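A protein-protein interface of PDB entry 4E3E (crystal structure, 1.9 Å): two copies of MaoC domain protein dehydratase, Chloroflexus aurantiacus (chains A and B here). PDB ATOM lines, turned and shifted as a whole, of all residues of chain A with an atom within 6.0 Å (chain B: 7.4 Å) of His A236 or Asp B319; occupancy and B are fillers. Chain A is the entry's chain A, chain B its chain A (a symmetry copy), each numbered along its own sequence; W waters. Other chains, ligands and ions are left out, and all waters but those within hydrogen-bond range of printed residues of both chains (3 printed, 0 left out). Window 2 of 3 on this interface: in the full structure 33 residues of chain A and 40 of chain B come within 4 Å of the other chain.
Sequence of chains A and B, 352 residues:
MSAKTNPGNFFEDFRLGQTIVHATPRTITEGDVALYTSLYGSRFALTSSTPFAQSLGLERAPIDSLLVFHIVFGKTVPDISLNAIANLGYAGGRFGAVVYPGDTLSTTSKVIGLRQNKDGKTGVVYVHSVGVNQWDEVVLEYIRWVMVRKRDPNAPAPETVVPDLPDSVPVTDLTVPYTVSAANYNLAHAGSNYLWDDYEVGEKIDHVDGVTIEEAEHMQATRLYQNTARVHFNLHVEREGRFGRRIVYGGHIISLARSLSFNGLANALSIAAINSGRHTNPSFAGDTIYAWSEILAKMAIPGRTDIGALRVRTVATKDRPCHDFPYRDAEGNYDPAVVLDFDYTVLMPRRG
The side-chain amide oxygen (OD1) of Asn A234 is in hydrogen-bond range of the backbone NH (N) of His A236 (3.0 Å).
The backbone carbonyl oxygen (O) of Thr B288 lies within hydrogen-bond range of the backbone NH (N) of Asp B319, 2.8 Å away.
OD1 of Asn A234 is in hydrogen-bond range of N of Val A237, at 2.8 Å.
O of Tyr B290 is in hydrogen-bond range of N of Thr B317 (2.9 Å).
The side-chain hydroxyl (OG1) of Thr B212 is in hydrogen-bond range of the side-chain hydroxyl (OG1) of Thr B288, at 2.8 Å.
No position is printed for both chains.
Of the 10 pairs that touch across the chains among the printed residues, none has its exchanged pair printed and touching as well.
Among the printed residues, merely in contact across the chains: His A236 with Tyr B290, Asn A234 with Thr B288, Val A237 with Tyr B290, Asn A234 with Thr B212 and His A236 with Arg B320.
Printed residues of chain B that touch a printed residue of chain A: Gly B210, Thr B212, Thr B288, Tyr B290, Asp B319 and Arg B320.
Hydrophobic or aromatic side chains of chain B within 4 Å of the printed part of chain A: Tyr B290.
Among the printed residues, 10 pairs touch across the chains.
Among the printed residues, no Asp or Glu carboxylate lies within 4 Å of a Lys or Arg side-chain nitrogen of the other chain.
The side-chain amide nitrogen (ND2) of Asn A234 lies within hydrogen-bond range of the side-chain hydroxyl (OH) of Tyr B290.
The backbone NH of Leu A235 lies within hydrogen-bond range of the side-chain hydroxyl of Thr B212 (2.8 Å).
O of Gly B210 sits at hydrogen-bond distance from ND2 of Asn A234 (3.4 Å).
The backbone carbonyl oxygen (O) of Asp B319 lies within hydrogen-bond range of a ring nitrogen (NE2) of His A236 (3.5 Å).
The backbone NH (N) of His A236 is in hydrogen-bond range of the side-chain hydroxyl (OG1) of Thr B288 (3.3 Å).
Water W3 lies within hydrogen-bond range of the side-chain hydroxyl (OG1) of Thr B288 (2.5 Å), the backbone carbonyl oxygen (O) of Gly B286 (2.8 Å), the side-chain carboxylate (OD1) of Asp B319 (2.9 Å) and the guanidinium group (NH2) of Arg A239 (3.4 Å).
Water W1 bridges O of Gly B286 and NH1 of Arg A239.
Water W2 lies within hydrogen-bond range of the backbone NH (N) of Gly B210 (2.8 Å) and the side-chain amide nitrogen (ND2) of Asn A234 (2.9 Å).
Of the printed residues of chain B, Asn A234 touches Gly B210 (3.4 Å), Thr B212 (3.8 Å), Thr B288 (3.4 Å) and Tyr B290 (3.1 Å).
Of the printed residues of chain B, Leu A235 touches Thr B212 (2.8 Å).
Printed residues of chain B within 4 Å of His A236: Thr B288 (3.3 Å), Tyr B290 (3.0 Å), Asp B319 (3.5 Å) and Arg B320 (3.8 Å).
Of chain A, only His A236 (3.5 Å) comes within 4 Å of Asp B319.
The nearest printed residue of chain B that does not touch His A236 is Thr B212 (4.2 Å).
The nearest printed residue of chain A that does not touch Tyr B290 is Leu A235 (6.7 Å).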
ATOM      1  N   ASN A 234     -28.207  33.560   5.277  1.00  0.00           N
ATOM      2  CA  ASN A 234     -27.426  32.764   4.350  1.00  0.00           C
ATOM      3  C   ASN A 234     -27.334  33.377   2.970  1.00  0.00           C
ATOM      4  O   ASN A 234     -28.203  33.166   2.116  1.00  0.00           O
ATOM      5  CB  ASN A 234     -28.007  31.343   4.264  1.00  0.00           C
ATOM      6  CG  ASN A 234     -27.065  30.365   3.592  1.00  0.00           C
ATOM      7  OD1 ASN A 234     -26.326  30.729   2.674  1.00  0.00           O
ATOM      8  ND2 ASN A 234     -27.091  29.107   4.043  1.00  0.00           N
ATOM      9  N   LEU A 235     -26.254  34.114   2.750  1.00  0.00           N
ATOM     10  CA  LEU A 235     -26.018  34.753   1.465  1.00  0.00           C
ATOM     11  C   LEU A 235     -25.709  33.716   0.393  1.00  0.00           C
ATOM     12  O   LEU A 235     -26.114  33.882  -0.753  1.00  0.00           O
ATOM     13  CB  LEU A 235     -24.891  35.789   1.559  1.00  0.00           C
ATOM     14  CG  LEU A 235     -24.566  36.588   0.283  1.00  0.00           C
ATOM     15  CD1 LEU A 235     -25.790  37.337  -0.240  1.00  0.00           C
ATOM     16  CD2 LEU A 235     -23.394  37.543   0.521  1.00  0.00           C
ATOM     17  N   HIS A 236     -24.989  32.659   0.775  1.00  0.00           N
ATOM     18  CA  HIS A 236     -24.638  31.568  -0.137  1.00  0.00           C
ATOM     19  C   HIS A 236     -25.880  31.030  -0.802  1.00  0.00           C
ATOM     20  O   HIS A 236     -25.897  30.817  -2.019  1.00  0.00           O
ATOM     21  CB  HIS A 236     -23.877  30.470   0.617  1.00  0.00           C
ATOM     22  CG  HIS A 236     -23.476  29.290  -0.236  1.00  0.00           C
ATOM     23  ND1 HIS A 236     -22.904  29.428  -1.451  1.00  0.00           N
ATOM     24  CD2 HIS A 236     -23.554  27.924   0.009  1.00  0.00           C
ATOM     25  CE1 HIS A 236     -22.647  28.211  -1.967  1.00  0.00           C
ATOM     26  NE2 HIS A 236     -23.040  27.291  -1.068  1.00  0.00           N
ATOM     27  N   VAL A 237     -26.944  30.848  -0.018  1.00  0.00           N
ATOM     28  CA  VAL A 237     -28.226  30.381  -0.568  1.00  0.00           C
ATOM     29  C   VAL A 237     -29.040  31.526  -1.159  1.00  0.00           C
ATOM     30  O   VAL A 237     -29.519  31.436  -2.299  1.00  0.00           O
ATOM     31  CB  VAL A 237     -29.066  29.634   0.491  1.00  0.00           C
ATOM     32  CG1 VAL A 237     -30.495  29.393  -0.010  1.00  0.00           C
ATOM     33  CG2 VAL A 237     -28.387  28.306   0.839  1.00  0.00           C
ATOM     34  N   GLU A 238     -29.188  32.606  -0.394  1.00  0.00           N
ATOM     35  CA  GLU A 238     -30.097  33.676  -0.793  1.00  0.00           C
ATOM     36  C   GLU A 238     -29.640  34.383  -2.051  1.00  0.00           C
ATOM     37  O   GLU A 238     -30.472  34.919  -2.787  1.00  0.00           O
ATOM     38  CB  GLU A 238     -30.381  34.668   0.341  1.00  0.00           C
ATOM     39  CG  GLU A 238     -31.273  34.086   1.425  1.00  0.00           C
ATOM     40  CD  GLU A 238     -32.456  33.310   0.849  1.00  0.00           C
ATOM     41  OE1 GLU A 238     -33.188  33.847  -0.004  1.00  0.00           O
ATOM     42  OE2 GLU A 238     -32.649  32.149   1.242  1.00  0.00           O
ATOM     43  N   ARG A 239     -28.356  34.342  -2.317  1.00  0.00           N
ATOM     44  CA  ARG A 239     -27.787  34.982  -3.479  1.00  0.00           C
ATOM     45  C   ARG A 239     -28.288  34.320  -4.730  1.00  0.00           C
ATOM     46  O   ARG A 239     -28.336  34.931  -5.767  1.00  0.00           O
ATOM     47  CB  ARG A 239     -26.268  35.065  -3.403  1.00  0.00           C
ATOM     48  CG  ARG A 239     -25.510  34.367  -4.491  1.00  0.00           C
ATOM     49  CD  ARG A 239     -24.117  33.976  -4.051  1.00  0.00           C
ATOM     50  NE  ARG A 239     -23.268  35.120  -3.813  1.00  0.00           N
ATOM     51  CZ  ARG A 239     -22.314  35.170  -2.894  1.00  0.00           C
ATOM     52  NH1 ARG A 239     -21.616  36.272  -2.763  1.00  0.00           N
ATOM     53  NH2 ARG A 239     -22.068  34.132  -2.107  1.00  0.00           N
ATOM     54  N   GLU A 240     -28.632  33.055  -4.634  1.00  0.00           N
ATOM     55  CA  GLU A 240     -29.182  32.346  -5.794  1.00  0.00           C
ATOM     56  C   GLU A 240     -30.683  32.575  -5.903  1.00  0.00           C
ATOM     57  O   GLU A 240     -31.247  32.358  -6.958  1.00  0.00           O
ATOM     58  CB  GLU A 240     -28.861  30.842  -5.771  1.00  0.00           C
ATOM     59  CG  GLU A 240     -27.382  30.497  -5.611  1.00  0.00           C
ATOM     60  CD  GLU A 240     -26.482  31.133  -6.670  1.00  0.00           C
ATOM     61  OE1 GLU A 240     -26.875  31.193  -7.862  1.00  0.00           O
ATOM     62  OE2 GLU A 240     -25.365  31.562  -6.302  1.00  0.00           O
ATOM     63  N   GLY B 210     -26.470  27.532   7.204  1.00  0.00           N
ATOM     64  CA  GLY B 210     -25.292  28.324   6.860  1.00  0.00           C
ATOM     65  C   GLY B 210     -25.476  29.776   7.273  1.00  0.00           C
ATOM     66  O   GLY B 210     -26.575  30.319   7.142  1.00  0.00           O
ATOM     67  N   VAL B 211     -24.406  30.405   7.769  1.00  0.00           N
ATOM     68  CA  VAL B 211     -24.467  31.811   8.199  1.00  0.00           C
ATOM     69  C   VAL B 211     -23.326  32.627   7.606  1.00  0.00           C
ATOM     70  O   VAL B 211     -22.156  32.200   7.617  1.00  0.00           O
ATOM     71  CB  VAL B 211     -24.516  31.980   9.742  1.00  0.00           C
ATOM     72  CG1 VAL B 211     -25.784  31.348  10.299  1.00  0.00           C
ATOM     73  CG2 VAL B 211     -23.265  31.421  10.431  1.00  0.00           C
ATOM     74  N   THR B 212     -23.674  33.801   7.084  1.00  0.00           N
ATOM     75  CA  THR B 212     -22.693  34.656   6.414  1.00  0.00           C
ATOM     76  C   THR B 212     -22.050  35.629   7.405  1.00  0.00           C
ATOM     77  O   THR B 212     -22.743  36.260   8.204  1.00  0.00           O
ATOM     78  CB  THR B 212     -23.346  35.401   5.244  1.00  0.00           C
ATOM     79  OG1 THR B 212     -23.965  34.438   4.393  1.00  0.00           O
ATOM     80  CG2 THR B 212     -22.326  36.205   4.433  1.00  0.00           C
ATOM     81  N   GLY B 286     -18.223  37.811   4.200  1.00  0.00           N
ATOM     82  CA  GLY B 286     -18.781  37.359   2.921  1.00  0.00           C
ATOM     83  C   GLY B 286     -18.782  35.847   2.726  1.00  0.00           C
ATOM     84  O   GLY B 286     -19.466  35.320   1.835  1.00  0.00           O
ATOM     85  N   ASP B 287     -17.986  35.139   3.518  1.00  0.00           N
ATOM     86  CA  ASP B 287     -18.035  33.687   3.522  1.00  0.00           C
ATOM     87  C   ASP B 287     -19.249  33.211   4.291  1.00  0.00           C
ATOM     88  O   ASP B 287     -19.581  33.751   5.360  1.00  0.00           O
ATOM     89  CB  ASP B 287     -16.771  33.103   4.156  1.00  0.00           C
ATOM     90  CG  ASP B 287     -15.527  33.279   3.272  1.00  0.00           C
ATOM     91  OD1 ASP B 287     -15.658  33.528   2.054  1.00  0.00           O
ATOM     92  OD2 ASP B 287     -14.401  33.156   3.802  1.00  0.00           O
ATOM     93  N   THR B 288     -19.905  32.180   3.777  1.00  0.00           N
ATOM     94  CA  THR B 288     -20.995  31.534   4.544  1.00  0.00           C
ATOM     95  C   THR B 288     -20.513  30.248   5.219  1.00  0.00           C
ATOM     96  O   THR B 288     -20.050  29.326   4.548  1.00  0.00           O
ATOM     97  CB  THR B 288     -22.206  31.261   3.635  1.00  0.00           C
ATOM     98  OG1 THR B 288     -22.584  32.490   3.006  1.00  0.00           O
ATOM     99  CG2 THR B 288     -23.395  30.702   4.420  1.00  0.00           C
ATOM    100  N   ILE B 289     -20.641  30.185   6.547  1.00  0.00           N
ATOM    101  CA  ILE B 289     -20.100  29.081   7.315  1.00  0.00           C
ATOM    102  C   ILE B 289     -21.178  28.017   7.545  1.00  0.00           C
ATOM    103  O   ILE B 289     -22.301  28.335   7.987  1.00  0.00           O
ATOM    104  CB  ILE B 289     -19.568  29.550   8.701  1.00  0.00           C
ATOM    105  CG1 ILE B 289     -18.451  30.612   8.549  1.00  0.00           C
ATOM    106  CG2 ILE B 289     -19.072  28.358   9.512  1.00  0.00           C
ATOM    107  CD1 ILE B 289     -17.346  30.255   7.536  1.00  0.00           C
ATOM    108  N   TYR B 290     -20.823  26.764   7.244  1.00  0.00           N
ATOM    109  CA  TYR B 290     -21.641  25.592   7.549  1.00  0.00           C
ATOM    110  C   TYR B 290     -20.841  24.679   8.455  1.00  0.00           C
ATOM    111  O   TYR B 290     -19.622  24.817   8.559  1.00  0.00           O
ATOM    112  CB  TYR B 290     -21.924  24.814   6.282  1.00  0.00           C
ATOM    113  CG  TYR B 290     -22.776  25.514   5.271  1.00  0.00           C
ATOM    114  CD1 TYR B 290     -22.210  26.370   4.315  1.00  0.00           C
ATOM    115  CD2 TYR B 290     -24.151  25.281   5.228  1.00  0.00           C
ATOM    116  CE1 TYR B 290     -22.999  26.991   3.355  1.00  0.00           C
ATOM    117  CE2 TYR B 290     -24.950  25.892   4.274  1.00  0.00           C
ATOM    118  CZ  TYR B 290     -24.374  26.747   3.348  1.00  0.00           C
ATOM    119  OH  TYR B 290     -25.176  27.339   2.416  1.00  0.00           O
ATOM    120  N   THR B 317     -17.056  24.551   7.216  1.00  0.00           N
ATOM    121  CA  THR B 317     -16.717  24.762   5.830  1.00  0.00           C
ATOM    122  C   THR B 317     -17.284  26.073   5.369  1.00  0.00           C
ATOM    123  O   THR B 317     -18.178  26.591   5.960  1.00  0.00           O
ATOM    124  CB  THR B 317     -17.262  23.653   4.933  1.00  0.00           C
ATOM    125  OG1 THR B 317     -18.664  23.561   5.074  1.00  0.00           O
ATOM    126  CG2 THR B 317     -16.693  22.363   5.307  1.00  0.00           C
ATOM    127  N   LYS B 318     -16.753  26.600   4.289  1.00  0.00           N
ATOM    128  CA  LYS B 318     -17.322  27.778   3.712  1.00  0.00           C
ATOM    129  C   LYS B 318     -18.020  27.459   2.424  1.00  0.00           C
ATOM    130  O   LYS B 318     -17.512  26.737   1.616  1.00  0.00           O
ATOM    131  CB  LYS B 318     -16.303  28.891   3.517  1.00  0.00           C
ATOM    132  CG  LYS B 318     -15.104  28.544   2.683  1.00  0.00           C
ATOM    133  CD  LYS B 318     -14.453  29.787   2.130  1.00  0.00           C
ATOM    134  CE  LYS B 318     -13.243  30.128   2.941  1.00  0.00           C
ATOM    135  NZ  LYS B 318     -12.638  31.422   2.607  1.00  0.00           N
ATOM    136  N   ASP B 319     -19.211  27.988   2.276  1.00  0.00           N
ATOM    137  CA  ASP B 319     -19.935  27.896   1.055  1.00  0.00           C
ATOM    138  C   ASP B 319     -20.071  26.459   0.623  1.00  0.00           C
ATOM    139  O   ASP B 319     -19.826  26.138  -0.507  1.00  0.00           O
ATOM    140  CB  ASP B 319     -19.253  28.726  -0.015  1.00  0.00           C
ATOM    141  CG  ASP B 319     -19.130  30.178   0.360  1.00  0.00           C
ATOM    142  OD1 ASP B 319     -19.812  30.657   1.247  1.00  0.00           O
ATOM    143  OD2 ASP B 319     -18.331  30.862  -0.254  1.00  0.00           O
ATOM    144  N   ARG B 320     -20.451  25.604   1.550  1.00  0.00           N
ATOM    145  CA  ARG B 320     -20.454  24.136   1.429  1.00  0.00           C
ATOM    146  C   ARG B 320     -20.426  23.576   0.003  1.00  0.00           C
ATOM    147  O   ARG B 320     -21.324  23.858  -0.804  1.00  0.00           O
ATOM    148  CB  ARG B 320     -21.615  23.517   2.224  1.00  0.00           C
ATOM    149  CG  ARG B 320     -22.937  23.395   1.477  1.00  0.00           C
ATOM    150  CD  ARG B 320     -23.772  22.296   2.106  1.00  0.00           C
ATOM    151  NE  ARG B 320     -22.921  21.288   2.733  1.00  0.00           N
ATOM    152  CZ  ARG B 320     -23.377  20.242   3.414  1.00  0.00           C
ATOM    153  NH1 ARG B 320     -24.684  20.062   3.553  1.00  0.00           N
ATOM    154  NH2 ARG B 320     -22.527  19.375   3.956  1.00  0.00           N
ATOM    155  N   PRO B 321     -19.392  22.765  -0.312  1.00  0.00           N
ATOM    156  CA  PRO B 321     -19.285  22.151  -1.641  1.00  0.00           C
ATOM    157  C   PRO B 321     -20.287  20.999  -1.847  1.00  0.00           C
ATOM    158  O   PRO B 321     -21.090  20.708  -0.946  1.00  0.00           O
ATOM    159  CB  PRO B 321     -17.837  21.642  -1.675  1.00  0.00           C
ATOM    160  CG  PRO B 321     -17.494  21.388  -0.253  1.00  0.00           C
ATOM    161  CD  PRO B 321     -18.236  22.428   0.547  1.00  0.00           C
ATOM    162  N   CYS B 322     -20.261  20.383  -3.014  1.00  0.00           N
ATOM    163  CA  CYS B 322     -21.195  19.312  -3.328  1.00  0.00           C
ATOM    164  C   CYS B 322     -21.116  17.957  -2.558  1.00  0.00           C
ATOM    165  O   CYS B 322     -22.132  17.500  -2.065  1.00  0.00           O
ATOM    166  CB  CYS B 322     -21.214  19.136  -4.849  1.00  0.00           C
ATOM    167  SG  CYS B 322     -20.989  20.702  -5.738  1.00  0.00           S
ATOM    168  N   ALA B 337     -12.333  23.826   1.005  1.00  0.00           N
ATOM    169  CA  ALA B 337     -13.528  24.426   1.610  1.00  0.00           C
ATOM    170  C   ALA B 337     -13.535  24.380   3.142  1.00  0.00           C
ATOM    171  O   ALA B 337     -14.304  25.114   3.782  1.00  0.00           O
ATOM    172  CB  ALA B 337     -14.788  23.772   1.051  1.00  0.00           C
HETATM  173  O   HOH W   1     -20.003  36.812  -0.365  1.00  0.00           O
HETATM  174  O   HOH W   2     -28.954  28.221   6.014  1.00  0.00           O
HETATM  175  O   HOH W   3     -21.156  33.218   1.085  1.00  0.00           O
